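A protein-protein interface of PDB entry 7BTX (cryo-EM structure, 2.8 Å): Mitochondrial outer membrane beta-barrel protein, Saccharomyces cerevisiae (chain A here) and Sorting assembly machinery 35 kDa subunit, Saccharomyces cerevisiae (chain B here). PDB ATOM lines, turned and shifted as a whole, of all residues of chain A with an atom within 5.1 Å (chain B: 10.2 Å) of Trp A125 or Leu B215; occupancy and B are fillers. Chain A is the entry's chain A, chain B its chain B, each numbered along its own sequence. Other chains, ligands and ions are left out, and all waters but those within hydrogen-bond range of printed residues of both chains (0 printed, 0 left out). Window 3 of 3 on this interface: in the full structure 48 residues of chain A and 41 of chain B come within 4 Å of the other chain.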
ATOM      1  N   GLY A  85      -7.227  -8.646  -1.330  1.00  0.00           N
ATOM      2  CA  GLY A  85      -7.714  -8.546  -2.696  1.00  0.00           C
ATOM      3  C   GLY A  85      -8.525  -9.782  -3.036  1.00  0.00           C
ATOM      4  O   GLY A  85      -8.240 -10.865  -2.538  1.00  0.00           O
ATOM      5  N   GLN A  86      -9.547  -9.609  -3.866  1.00  0.00           N
ATOM      6  CA  GLN A  86     -10.444 -10.704  -4.210  1.00  0.00           C
ATOM      7  C   GLN A  86     -10.855 -10.589  -5.663  1.00  0.00           C
ATOM      8  O   GLN A  86     -11.443  -9.587  -6.064  1.00  0.00           O
ATOM      9  CB  GLN A  86     -11.687 -10.707  -3.326  1.00  0.00           C
ATOM     10  CG  GLN A  86     -11.502 -11.408  -2.013  1.00  0.00           C
ATOM     11  CD  GLN A  86     -12.712 -11.294  -1.133  1.00  0.00           C
ATOM     12  OE1 GLN A  86     -12.892 -12.079  -0.206  1.00  0.00           O
ATOM     13  NE2 GLN A  86     -13.553 -10.312  -1.412  1.00  0.00           N
ATOM     14  N   ARG A  87     -10.549 -11.619  -6.438  1.00  0.00           N
ATOM     15  CA  ARG A  87     -10.909 -11.707  -7.844  1.00  0.00           C
ATOM     16  C   ARG A  87     -11.695 -12.989  -8.032  1.00  0.00           C
ATOM     17  O   ARG A  87     -11.224 -14.059  -7.647  1.00  0.00           O
ATOM     18  CB  ARG A  87      -9.665 -11.736  -8.740  1.00  0.00           C
ATOM     19  CG  ARG A  87      -9.032 -10.406  -9.079  1.00  0.00           C
ATOM     20  CD  ARG A  87      -8.146  -9.876  -7.976  1.00  0.00           C
ATOM     21  NE  ARG A  87      -7.041 -10.762  -7.635  1.00  0.00           N
ATOM     22  CZ  ARG A  87      -6.274 -10.593  -6.565  1.00  0.00           C
ATOM     23  NH1 ARG A  87      -5.293 -11.420  -6.293  1.00  0.00           N
ATOM     24  NH2 ARG A  87      -6.489  -9.577  -5.761  1.00  0.00           N
ATOM     25  N   GLY A  88     -12.878 -12.902  -8.614  1.00  0.00           N
ATOM     26  CA  GLY A  88     -13.616 -14.116  -8.866  1.00  0.00           C
ATOM     27  C   GLY A  88     -14.991 -13.873  -9.426  1.00  0.00           C
ATOM     28  O   GLY A  88     -15.317 -12.773  -9.870  1.00  0.00           O
ATOM     29  N   THR A 123     -16.230 -19.023  -6.886  1.00  0.00           N
ATOM     30  CA  THR A 123     -14.800 -19.253  -7.016  1.00  0.00           C
ATOM     31  C   THR A 123     -14.095 -17.913  -6.881  1.00  0.00           C
ATOM     32  O   THR A 123     -14.530 -16.921  -7.464  1.00  0.00           O
ATOM     33  CB  THR A 123     -14.460 -19.905  -8.358  1.00  0.00           C
ATOM     34  OG1 THR A 123     -15.255 -21.082  -8.525  1.00  0.00           O
ATOM     35  CG2 THR A 123     -12.995 -20.314  -8.399  1.00  0.00           C
ATOM     36  N   CYS A 124     -13.021 -17.876  -6.102  1.00  0.00           N
ATOM     37  CA  CYS A 124     -12.363 -16.614  -5.799  1.00  0.00           C
ATOM     38  C   CYS A 124     -10.877 -16.839  -5.590  1.00  0.00           C
ATOM     39  O   CYS A 124     -10.484 -17.729  -4.836  1.00  0.00           O
ATOM     40  CB  CYS A 124     -12.977 -15.972  -4.553  1.00  0.00           C
ATOM     41  SG  CYS A 124     -12.278 -14.393  -4.075  1.00  0.00           S
ATOM     42  N   TRP A 125     -10.062 -16.030  -6.257  1.00  0.00           N
ATOM     43  CA  TRP A 125      -8.639 -15.926  -5.977  1.00  0.00           C
ATOM     44  C   TRP A 125      -8.456 -14.778  -4.994  1.00  0.00           C
ATOM     45  O   TRP A 125      -8.797 -13.635  -5.303  1.00  0.00           O
ATOM     46  CB  TRP A 125      -7.852 -15.703  -7.271  1.00  0.00           C
ATOM     47  CG  TRP A 125      -6.425 -15.202  -7.145  1.00  0.00           C
ATOM     48  CD1 TRP A 125      -5.529 -15.458  -6.144  1.00  0.00           C
ATOM     49  CD2 TRP A 125      -5.733 -14.383  -8.090  1.00  0.00           C
ATOM     50  NE1 TRP A 125      -4.345 -14.830  -6.395  1.00  0.00           N
ATOM     51  CE2 TRP A 125      -4.439 -14.169  -7.589  1.00  0.00           C
ATOM     52  CE3 TRP A 125      -6.086 -13.806  -9.310  1.00  0.00           C
ATOM     53  CZ2 TRP A 125      -3.502 -13.394  -8.261  1.00  0.00           C
ATOM     54  CZ3 TRP A 125      -5.156 -13.047  -9.974  1.00  0.00           C
ATOM     55  CH2 TRP A 125      -3.880 -12.845  -9.450  1.00  0.00           C
ATOM     56  N   ARG A 126      -7.917 -15.082  -3.819  1.00  0.00           N
ATOM     57  CA  ARG A 126      -7.796 -14.105  -2.750  1.00  0.00           C
ATOM     58  C   ARG A 126      -6.337 -13.888  -2.377  1.00  0.00           C
ATOM     59  O   ARG A 126      -5.634 -14.832  -2.011  1.00  0.00           O
ATOM     60  CB  ARG A 126      -8.588 -14.536  -1.522  1.00  0.00           C
ATOM     61  CG  ARG A 126      -8.402 -13.601  -0.356  1.00  0.00           C
ATOM     62  CD  ARG A 126      -9.521 -13.712   0.628  1.00  0.00           C
ATOM     63  NE  ARG A 126      -9.562 -15.019   1.260  1.00  0.00           N
ATOM     64  CZ  ARG A 126     -10.625 -15.505   1.881  1.00  0.00           C
ATOM     65  NH1 ARG A 126     -11.737 -14.793   1.943  1.00  0.00           N
ATOM     66  NH2 ARG A 126     -10.577 -16.699   2.440  1.00  0.00           N
ATOM     67  N   SER A 127      -5.895 -12.638  -2.454  1.00  0.00           N
ATOM     68  CA  SER A 127      -4.572 -12.226  -2.012  1.00  0.00           C
ATOM     69  C   SER A 127      -4.676 -11.535  -0.662  1.00  0.00           C
ATOM     70  O   SER A 127      -5.595 -10.750  -0.429  1.00  0.00           O
ATOM     71  CB  SER A 127      -3.926 -11.283  -3.021  1.00  0.00           C
ATOM     72  OG  SER A 127      -3.587 -11.969  -4.206  1.00  0.00           O
ATOM     73  N   ASP A 151      -1.389 -15.869  -1.558  1.00  0.00           N
ATOM     74  CA  ASP A 151      -2.469 -16.043  -2.512  1.00  0.00           C
ATOM     75  C   ASP A 151      -3.136 -17.383  -2.268  1.00  0.00           C
ATOM     76  O   ASP A 151      -2.471 -18.358  -1.920  1.00  0.00           O
ATOM     77  CB  ASP A 151      -1.951 -15.992  -3.949  1.00  0.00           C
ATOM     78  CG  ASP A 151      -1.311 -14.673  -4.295  1.00  0.00           C
ATOM     79  OD1 ASP A 151      -2.043 -13.730  -4.645  1.00  0.00           O
ATOM     80  OD2 ASP A 151      -0.072 -14.578  -4.229  1.00  0.00           O
ATOM     81  N   GLN A 152      -4.450 -17.434  -2.445  1.00  0.00           N
ATOM     82  CA  GLN A 152      -5.137 -18.711  -2.413  1.00  0.00           C
ATOM     83  C   GLN A 152      -6.274 -18.700  -3.417  1.00  0.00           C
ATOM     84  O   GLN A 152      -6.772 -17.646  -3.803  1.00  0.00           O
ATOM     85  CB  GLN A 152      -5.667 -19.060  -1.022  1.00  0.00           C
ATOM     86  CG  GLN A 152      -6.957 -18.403  -0.639  1.00  0.00           C
ATOM     87  CD  GLN A 152      -7.498 -18.945   0.659  1.00  0.00           C
ATOM     88  OE1 GLN A 152      -6.827 -19.705   1.352  1.00  0.00           O
ATOM     89  NE2 GLN A 152      -8.735 -18.600   0.969  1.00  0.00           N
ATOM     90  N   LEU A 153      -6.646 -19.890  -3.866  1.00  0.00           N
ATOM     91  CA  LEU A 153      -7.790 -20.092  -4.734  1.00  0.00           C
ATOM     92  C   LEU A 153      -8.772 -21.006  -4.023  1.00  0.00           C
ATOM     93  O   LEU A 153      -8.369 -21.950  -3.343  1.00  0.00           O
ATOM     94  CB  LEU A 153      -7.368 -20.700  -6.069  1.00  0.00           C
ATOM     95  CG  LEU A 153      -8.384 -20.758  -7.201  1.00  0.00           C
ATOM     96  CD1 LEU A 153      -8.725 -19.376  -7.674  1.00  0.00           C
ATOM     97  CD2 LEU A 153      -7.816 -21.569  -8.333  1.00  0.00           C
ATOM     98  N   SER B 119       5.346 -15.708   2.169  1.00  0.00           N
ATOM     99  CA  SER B 119       4.916 -15.049   0.954  1.00  0.00           C
ATOM    100  C   SER B 119       5.512 -13.653   0.902  1.00  0.00           C
ATOM    101  O   SER B 119       5.891 -13.092   1.929  1.00  0.00           O
ATOM    102  CB  SER B 119       3.402 -14.966   0.886  1.00  0.00           C
ATOM    103  OG  SER B 119       2.993 -14.114  -0.159  1.00  0.00           O
ATOM    104  N   ARG B 120       5.596 -13.104  -0.314  1.00  0.00           N
ATOM    105  CA  ARG B 120       6.074 -11.737  -0.512  1.00  0.00           C
ATOM    106  C   ARG B 120       5.185 -10.726   0.207  1.00  0.00           C
ATOM    107  O   ARG B 120       5.662  -9.686   0.666  1.00  0.00           O
ATOM    108  CB  ARG B 120       6.128 -11.429  -2.011  1.00  0.00           C
ATOM    109  CG  ARG B 120       4.781 -11.671  -2.652  1.00  0.00           C
ATOM    110  CD  ARG B 120       4.643 -11.500  -4.102  1.00  0.00           C
ATOM    111  NE  ARG B 120       3.322 -11.989  -4.463  1.00  0.00           N
ATOM    112  CZ  ARG B 120       2.318 -11.226  -4.870  1.00  0.00           C
ATOM    113  NH1 ARG B 120       2.476  -9.924  -4.993  1.00  0.00           N
ATOM    114  NH2 ARG B 120       1.153 -11.770  -5.168  1.00  0.00           N
ATOM    115  N   LEU B 121       3.905 -11.046   0.373  1.00  0.00           N
ATOM    116  CA  LEU B 121       2.826 -10.239   0.883  1.00  0.00           C
ATOM    117  C   LEU B 121       2.814 -10.156   2.371  1.00  0.00           C
ATOM    118  O   LEU B 121       1.894  -9.618   2.952  1.00  0.00           O
ATOM    119  CB  LEU B 121       1.513 -10.804   0.351  1.00  0.00           C
ATOM    120  CG  LEU B 121       1.302 -10.719  -1.162  1.00  0.00           C
ATOM    121  CD1 LEU B 121      -0.122 -11.044  -1.542  1.00  0.00           C
ATOM    122  CD2 LEU B 121       1.682  -9.349  -1.686  1.00  0.00           C
ATOM    123  N   ASP B 185       6.908 -20.280 -16.450  1.00  0.00           N
ATOM    124  CA  ASP B 185       6.205 -19.913 -15.227  1.00  0.00           C
ATOM    125  C   ASP B 185       6.327 -20.966 -14.139  1.00  0.00           C
ATOM    126  O   ASP B 185       6.281 -20.614 -12.963  1.00  0.00           O
ATOM    127  CB  ASP B 185       4.728 -19.660 -15.504  1.00  0.00           C
ATOM    128  CG  ASP B 185       4.491 -18.398 -16.294  1.00  0.00           C
ATOM    129  OD1 ASP B 185       5.326 -17.484 -16.211  1.00  0.00           O
ATOM    130  OD2 ASP B 185       3.461 -18.315 -16.988  1.00  0.00           O
ATOM    131  N   PHE B 188       9.708 -20.356 -12.458  1.00  0.00           N
ATOM    132  CA  PHE B 188       9.662 -19.169 -11.613  1.00  0.00           C
ATOM    133  C   PHE B 188       8.959 -19.454 -10.293  1.00  0.00           C
ATOM    134  O   PHE B 188       9.483 -19.124  -9.224  1.00  0.00           O
ATOM    135  CB  PHE B 188       8.969 -18.016 -12.338  1.00  0.00           C
ATOM    136  CG  PHE B 188       8.727 -16.824 -11.461  1.00  0.00           C
ATOM    137  CD1 PHE B 188       9.774 -15.994 -11.110  1.00  0.00           C
ATOM    138  CD2 PHE B 188       7.463 -16.545 -10.967  1.00  0.00           C
ATOM    139  CE1 PHE B 188       9.563 -14.916 -10.288  1.00  0.00           C
ATOM    140  CE2 PHE B 188       7.256 -15.476 -10.140  1.00  0.00           C
ATOM    141  CZ  PHE B 188       8.304 -14.657  -9.804  1.00  0.00           C
ATOM    142  N   MET B 189       7.768 -20.055 -10.346  1.00  0.00           N
ATOM    143  CA  MET B 189       6.986 -20.335  -9.150  1.00  0.00           C
ATOM    144  C   MET B 189       7.595 -21.425  -8.286  1.00  0.00           C
ATOM    145  O   MET B 189       7.251 -21.524  -7.108  1.00  0.00           O
ATOM    146  CB  MET B 189       5.560 -20.727  -9.531  1.00  0.00           C
ATOM    147  CG  MET B 189       4.794 -19.666 -10.290  1.00  0.00           C
ATOM    148  SD  MET B 189       4.432 -18.194  -9.350  1.00  0.00           S
ATOM    149  CE  MET B 189       2.948 -18.710  -8.521  1.00  0.00           C
ATOM    150  N   SER B 193       7.831 -18.769  -4.977  1.00  0.00           N
ATOM    151  CA  SER B 193       6.483 -18.901  -4.452  1.00  0.00           C
ATOM    152  C   SER B 193       6.460 -19.951  -3.357  1.00  0.00           C
ATOM    153  O   SER B 193       7.122 -20.984  -3.461  1.00  0.00           O
ATOM    154  CB  SER B 193       5.495 -19.275  -5.551  1.00  0.00           C
ATOM    155  OG  SER B 193       4.189 -19.365  -5.042  1.00  0.00           O
ATOM    156  N   GLN B 195       3.567 -21.334  -2.634  1.00  0.00           N
ATOM    157  CA  GLN B 195       2.482 -22.222  -3.024  1.00  0.00           C
ATOM    158  C   GLN B 195       3.010 -23.632  -3.253  1.00  0.00           C
ATOM    159  O   GLN B 195       4.157 -23.822  -3.659  1.00  0.00           O
ATOM    160  CB  GLN B 195       1.801 -21.708  -4.289  1.00  0.00           C
ATOM    161  CG  GLN B 195       1.135 -20.355  -4.156  1.00  0.00           C
ATOM    162  CD  GLN B 195       0.760 -19.778  -5.496  1.00  0.00           C
ATOM    163  OE1 GLN B 195       0.634 -20.503  -6.471  1.00  0.00           O
ATOM    164  NE2 GLN B 195       0.595 -18.470  -5.556  1.00  0.00           N
ATOM    165  N   VAL B 207      -5.744 -29.634  -9.137  1.00  0.00           N
ATOM    166  CA  VAL B 207      -6.209 -28.905 -10.311  1.00  0.00           C
ATOM    167  C   VAL B 207      -6.248 -27.411 -10.029  1.00  0.00           C
ATOM    168  O   VAL B 207      -5.833 -26.601 -10.865  1.00  0.00           O
ATOM    169  CB  VAL B 207      -7.586 -29.434 -10.753  1.00  0.00           C
ATOM    170  CG1 VAL B 207      -8.101 -28.675 -11.962  1.00  0.00           C
ATOM    171  CG2 VAL B 207      -7.512 -30.913 -11.044  1.00  0.00           C
ATOM    172  N   GLU B 208      -6.728 -27.014  -8.850  1.00  0.00           N
ATOM    173  CA  GLU B 208      -6.786 -25.590  -8.553  1.00  0.00           C
ATOM    174  C   GLU B 208      -5.487 -25.069  -7.962  1.00  0.00           C
ATOM    175  O   GLU B 208      -5.301 -23.852  -7.894  1.00  0.00           O
ATOM    176  CB  GLU B 208      -7.930 -25.263  -7.600  1.00  0.00           C
ATOM    177  CG  GLU B 208      -7.668 -25.607  -6.163  1.00  0.00           C
ATOM    178  CD  GLU B 208      -8.781 -25.139  -5.263  1.00  0.00           C
ATOM    179  OE1 GLU B 208      -9.806 -24.653  -5.788  1.00  0.00           O
ATOM    180  OE2 GLU B 208      -8.618 -25.220  -4.031  1.00  0.00           O
ATOM    181  N   ASN B 209      -4.595 -25.951  -7.518  1.00  0.00           N
ATOM    182  CA  ASN B 209      -3.240 -25.520  -7.218  1.00  0.00           C
ATOM    183  C   ASN B 209      -2.456 -25.268  -8.491  1.00  0.00           C
ATOM    184  O   ASN B 209      -1.502 -24.485  -8.484  1.00  0.00           O
ATOM    185  CB  ASN B 209      -2.525 -26.564  -6.366  1.00  0.00           C
ATOM    186  CG  ASN B 209      -2.954 -26.530  -4.929  1.00  0.00           C
ATOM    187  OD1 ASN B 209      -3.827 -25.754  -4.550  1.00  0.00           O
ATOM    188  ND2 ASN B 209      -2.341 -27.371  -4.110  1.00  0.00           N
ATOM    189  N   SER B 210      -2.837 -25.927  -9.582  1.00  0.00           N
ATOM    190  CA  SER B 210      -2.232 -25.648 -10.876  1.00  0.00           C
ATOM    191  C   SER B 210      -2.813 -24.389 -11.498  1.00  0.00           C
ATOM    192  O   SER B 210      -2.202 -23.807 -12.398  1.00  0.00           O
ATOM    193  CB  SER B 210      -2.420 -26.844 -11.804  1.00  0.00           C
ATOM    194  OG  SER B 210      -1.950 -26.560 -13.107  1.00  0.00           O
ATOM    195  N   LEU B 211      -3.980 -23.953 -11.038  1.00  0.00           N
ATOM    196  CA  LEU B 211      -4.591 -22.727 -11.525  1.00  0.00           C
ATOM    197  C   LEU B 211      -4.152 -21.493 -10.755  1.00  0.00           C
ATOM    198  O   LEU B 211      -4.220 -20.393 -11.305  1.00  0.00           O
ATOM    199  CB  LEU B 211      -6.113 -22.836 -11.473  1.00  0.00           C
ATOM    200  CG  LEU B 211      -6.733 -23.817 -12.458  1.00  0.00           C
ATOM    201  CD1 LEU B 211      -8.228 -23.891 -12.247  1.00  0.00           C
ATOM    202  CD2 LEU B 211      -6.407 -23.408 -13.877  1.00  0.00           C
ATOM    203  N   LEU B 212      -3.731 -21.637  -9.497  1.00  0.00           N
ATOM    204  CA  LEU B 212      -3.072 -20.536  -8.809  1.00  0.00           C
ATOM    205  C   LEU B 212      -1.725 -20.199  -9.416  1.00  0.00           C
ATOM    206  O   LEU B 212      -1.337 -19.030  -9.435  1.00  0.00           O
ATOM    207  CB  LEU B 212      -2.853 -20.855  -7.336  1.00  0.00           C
ATOM    208  CG  LEU B 212      -3.679 -20.166  -6.270  1.00  0.00           C
ATOM    209  CD1 LEU B 212      -3.136 -20.594  -4.942  1.00  0.00           C
ATOM    210  CD2 LEU B 212      -3.608 -18.667  -6.426  1.00  0.00           C
ATOM    211  N   GLN B 213      -0.991 -21.199  -9.895  1.00  0.00           N
ATOM    212  CA  GLN B 213       0.322 -20.942 -10.459  1.00  0.00           C
ATOM    213  C   GLN B 213       0.246 -20.302 -11.834  1.00  0.00           C
ATOM    214  O   GLN B 213       1.264 -19.821 -12.332  1.00  0.00           O
ATOM    215  CB  GLN B 213       1.117 -22.238 -10.530  1.00  0.00           C
ATOM    216  CG  GLN B 213       1.630 -22.695  -9.193  1.00  0.00           C
ATOM    217  CD  GLN B 213       2.996 -23.319  -9.287  1.00  0.00           C
ATOM    218  OE1 GLN B 213       3.537 -23.493 -10.378  1.00  0.00           O
ATOM    219  NE2 GLN B 213       3.568 -23.658  -8.139  1.00  0.00           N
ATOM    220  N   LYS B 214      -0.922 -20.302 -12.464  1.00  0.00           N
ATOM    221  CA  LYS B 214      -1.119 -19.592 -13.715  1.00  0.00           C
ATOM    222  C   LYS B 214      -1.822 -18.263 -13.529  1.00  0.00           C
ATOM    223  O   LYS B 214      -1.579 -17.331 -14.300  1.00  0.00           O
ATOM    224  CB  LYS B 214      -1.922 -20.455 -14.691  1.00  0.00           C
ATOM    225  CG  LYS B 214      -1.310 -21.809 -14.948  1.00  0.00           C
ATOM    226  CD  LYS B 214      -2.136 -22.604 -15.933  1.00  0.00           C
ATOM    227  CE  LYS B 214      -1.347 -23.777 -16.485  1.00  0.00           C
ATOM    228  NZ  LYS B 214      -0.812 -24.643 -15.404  1.00  0.00           N
ATOM    229  N   LEU B 215      -2.693 -18.155 -12.528  1.00  0.00           N
ATOM    230  CA  LEU B 215      -3.368 -16.893 -12.269  1.00  0.00           C
ATOM    231  C   LEU B 215      -2.430 -15.893 -11.618  1.00  0.00           C
ATOM    232  O   LEU B 215      -2.439 -14.707 -11.960  1.00  0.00           O
ATOM    233  CB  LEU B 215      -4.582 -17.121 -11.375  1.00  0.00           C
ATOM    234  CG  LEU B 215      -5.896 -17.529 -12.025  1.00  0.00           C
ATOM    235  CD1 LEU B 215      -6.877 -17.927 -10.952  1.00  0.00           C
ATOM    236  CD2 LEU B 215      -6.444 -16.394 -12.857  1.00  0.00           C
ATOM    237  N   SER B 216      -1.611 -16.354 -10.680  1.00  0.00           N
ATOM    238  CA  SER B 216      -0.861 -15.468  -9.812  1.00  0.00           C
ATOM    239  C   SER B 216       0.607 -15.348 -10.184  1.00  0.00           C
ATOM    240  O   SER B 216       1.344 -14.670  -9.474  1.00  0.00           O
ATOM    241  CB  SER B 216      -0.985 -15.933  -8.363  1.00  0.00           C
ATOM    242  OG  SER B 216      -0.390 -17.199  -8.190  1.00  0.00           O
ATOM    243  N   ALA B 217       1.047 -15.966 -11.282  1.00  0.00           N
ATOM    244  CA  ALA B 217       2.469 -15.942 -11.619  1.00  0.00           C
ATOM    245  C   ALA B 217       2.931 -14.554 -12.035  1.00  0.00           C
ATOM    246  O   ALA B 217       4.061 -14.161 -11.737  1.00  0.00           O
ATOM    247  CB  ALA B 217       2.768 -16.944 -12.728  1.00  0.00           C
ATOM    248  N   LYS B 218       2.065 -13.793 -12.704  1.00  0.00           N
ATOM    249  CA  LYS B 218       2.450 -12.475 -13.189  1.00  0.00           C
ATOM    250  C   LYS B 218       2.524 -11.453 -12.065  1.00  0.00           C
ATOM    251  O   LYS B 218       3.406 -10.591 -12.077  1.00  0.00           O
ATOM    252  CB  LYS B 218       1.468 -12.022 -14.264  1.00  0.00           C
ATOM    253  CG  LYS B 218       1.788 -10.694 -14.908  1.00  0.00           C
ATOM    254  CD  LYS B 218       0.670 -10.283 -15.818  1.00  0.00           C
ATOM    255  CE  LYS B 218       0.767  -8.826 -16.192  1.00  0.00           C
ATOM    256  NZ  LYS B 218      -0.367  -8.391 -17.053  1.00  0.00           N
ATOM    257  N   SER B 219       1.627 -11.533 -11.086  1.00  0.00           N
ATOM    258  CA  SER B 219       1.665 -10.631  -9.944  1.00  0.00           C
ATOM    259  C   SER B 219       2.843 -10.898  -9.021  1.00  0.00           C
ATOM    260  O   SER B 219       3.304  -9.975  -8.348  1.00  0.00           O
ATOM    261  CB  SER B 219       0.365 -10.732  -9.152  1.00  0.00           C
ATOM    262  OG  SER B 219       0.287 -11.962  -8.466  1.00  0.00           O
ATOM    263  N   LEU B 220       3.335 -12.130  -8.974  1.00  0.00           N
ATOM    264  CA  LEU B 220       4.551 -12.430  -8.238  1.00  0.00           C
ATOM    265  C   LEU B 220       5.788 -11.951  -8.979  1.00  0.00           C
ATOM    266  O   LEU B 220       6.800 -11.638  -8.346  1.00  0.00           O
ATOM    267  CB  LEU B 220       4.647 -13.931  -7.979  1.00  0.00           C
ATOM    268  CG  LEU B 220       4.122 -14.497  -6.662  1.00  0.00           C
ATOM    269  CD1 LEU B 220       2.635 -14.489  -6.560  1.00  0.00           C
ATOM    270  CD2 LEU B 220       4.581 -15.876  -6.541  1.00  0.00           C
ATOM    271  N   LYS B 221       5.728 -11.898 -10.310  1.00  0.00           N
ATOM    272  CA  LYS B 221       6.825 -11.361 -11.103  1.00  0.00           C
ATOM    273  C   LYS B 221       6.912  -9.850 -10.980  1.00  0.00           C
ATOM    274  O   LYS B 221       8.008  -9.286 -11.000  1.00  0.00           O
ATOM    275  CB  LYS B 221       6.656 -11.749 -12.568  1.00  0.00           C
ATOM    276  CG  LYS B 221       6.997 -13.175 -12.871  1.00  0.00           C
ATOM    277  CD  LYS B 221       6.738 -13.514 -14.305  1.00  0.00           C
ATOM    278  CE  LYS B 221       6.647 -14.999 -14.479  1.00  0.00           C
ATOM    279  NZ  LYS B 221       7.227 -15.455 -15.757  1.00  0.00           N
ATOM    280  N   ILE B 222       5.765  -9.183 -10.865  1.00  0.00           N
ATOM    281  CA  ILE B 222       5.736  -7.732 -10.760  1.00  0.00           C
ATOM    282  C   ILE B 222       6.255  -7.280  -9.399  1.00  0.00           C
ATOM    283  O   ILE B 222       6.935  -6.254  -9.295  1.00  0.00           O
ATOM    284  CB  ILE B 222       4.302  -7.251 -11.065  1.00  0.00           C
ATOM    285  CG1 ILE B 222       4.046  -7.322 -12.566  1.00  0.00           C
ATOM    286  CG2 ILE B 222       4.036  -5.844 -10.579  1.00  0.00           C
ATOM    287  CD1 ILE B 222       2.599  -7.387 -12.925  1.00  0.00           C
ATOM    288  N   SER B 223       6.004  -8.061  -8.351  1.00  0.00           N
ATOM    289  CA  SER B 223       6.524  -7.722  -7.032  1.00  0.00           C
ATOM    290  C   SER B 223       8.029  -7.917  -6.943  1.00  0.00           C
ATOM    291  O   SER B 223       8.691  -7.240  -6.150  1.00  0.00           O
ATOM    292  CB  SER B 223       5.832  -8.562  -5.966  1.00  0.00           C
ATOM    293  OG  SER B 223       4.527  -8.097  -5.712  1.00  0.00           O
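No residue of chain B comes within 4 Å of Arg A87.
Of the printed residues of chain B, Trp A125 touches Leu B212 (3.8 Å), Leu B215 (3.4 Å) and Ser B216 (3.6 Å).
Arg A126 touches none of the printed residues of chain B.
Asp A151 touches just these residues of chain B: Arg B120 (3.2 Å), Gln B195 (3.9 Å), Leu B212 (3.8 Å) and Leu B220 (3.6 Å).
Of the printed residues of chain B, Leu A153 touches Glu B208 (3.4 Å), Leu B211 (3.8 Å) and Leu B212 (3.7 Å).
Of the printed residues of chain A, Leu B212 touches Trp A125, Asp A151, Gln A152 and Leu A153.
Of chain A, only Trp A125 comes within 4 Å of Leu B215.
Printed residues of chain A within 4 Å of Ser B216: Trp A125 (3.6 Å).
The nearest printed residue of chain A that does not touch Leu B220 is Trp A125 (6.5 Å).
The backbone carbonyl oxygen (O) of Leu B212 lies within hydrogen-bond range of the side-chain hydroxyl (OG) of Ser B216, 2.4 Å away.
The backbone carbonyl oxygen of Ser B216 sits at hydrogen-bond distance from the side-chain hydroxyl of Ser B219 (3.1 Å).
The side-chain carboxylate of Asp A151 is in hydrogen-bond range of the indole nitrogen of Trp A125, at 3.1 Å.
The backbone carbonyl oxygen (O) of Arg A87 sits at hydrogen-bond distance from the backbone NH (N) of Trp A125 (2.7 Å).
The backbone carbonyl oxygen (O) of Gln A152 sits at hydrogen-bond distance from the backbone NH (N) of Arg A126.
The side-chain hydroxyl (OG) of Ser B193 lies within hydrogen-bond range of the backbone NH (N) of Gln B195 (3.2 Å).
Hydrophobic or aromatic side chains of chain B within 4 Å of the printed part of chain A: Leu B211, Leu B212 and Leu B220.
Among the printed residues, Asp or Glu carboxylates within 4 Å of a Lys or Arg side-chain nitrogen of the other chain: Asp A151 with Arg B120 (3.2 Å).
The side-chain carboxylate of Asp A151 lies within salt-bridge range of the guanidinium group of Arg B120 (3.2 Å).
The backbone carbonyl oxygen of Leu A153 lies close to the side-chain carboxylate of Glu B208 (3.4 Å).
Among the printed residues, merely in contact across the chains: Trp A125 with Leu B212 (3.8 Å), Trp A125 with Leu B215 (3.4 Å), Trp A125 with Ser B216 (3.6 Å), Asp A151 with Gln B195 (3.9 Å), Asp A151 with Leu B212 (3.8 Å), Asp A151 with Leu B220 (3.6 Å), Gln A152 with Leu B212 (3.7 Å), Leu A153 with Leu B211 (3.8 Å) and Leu A153 with Leu B212 (3.7 Å).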
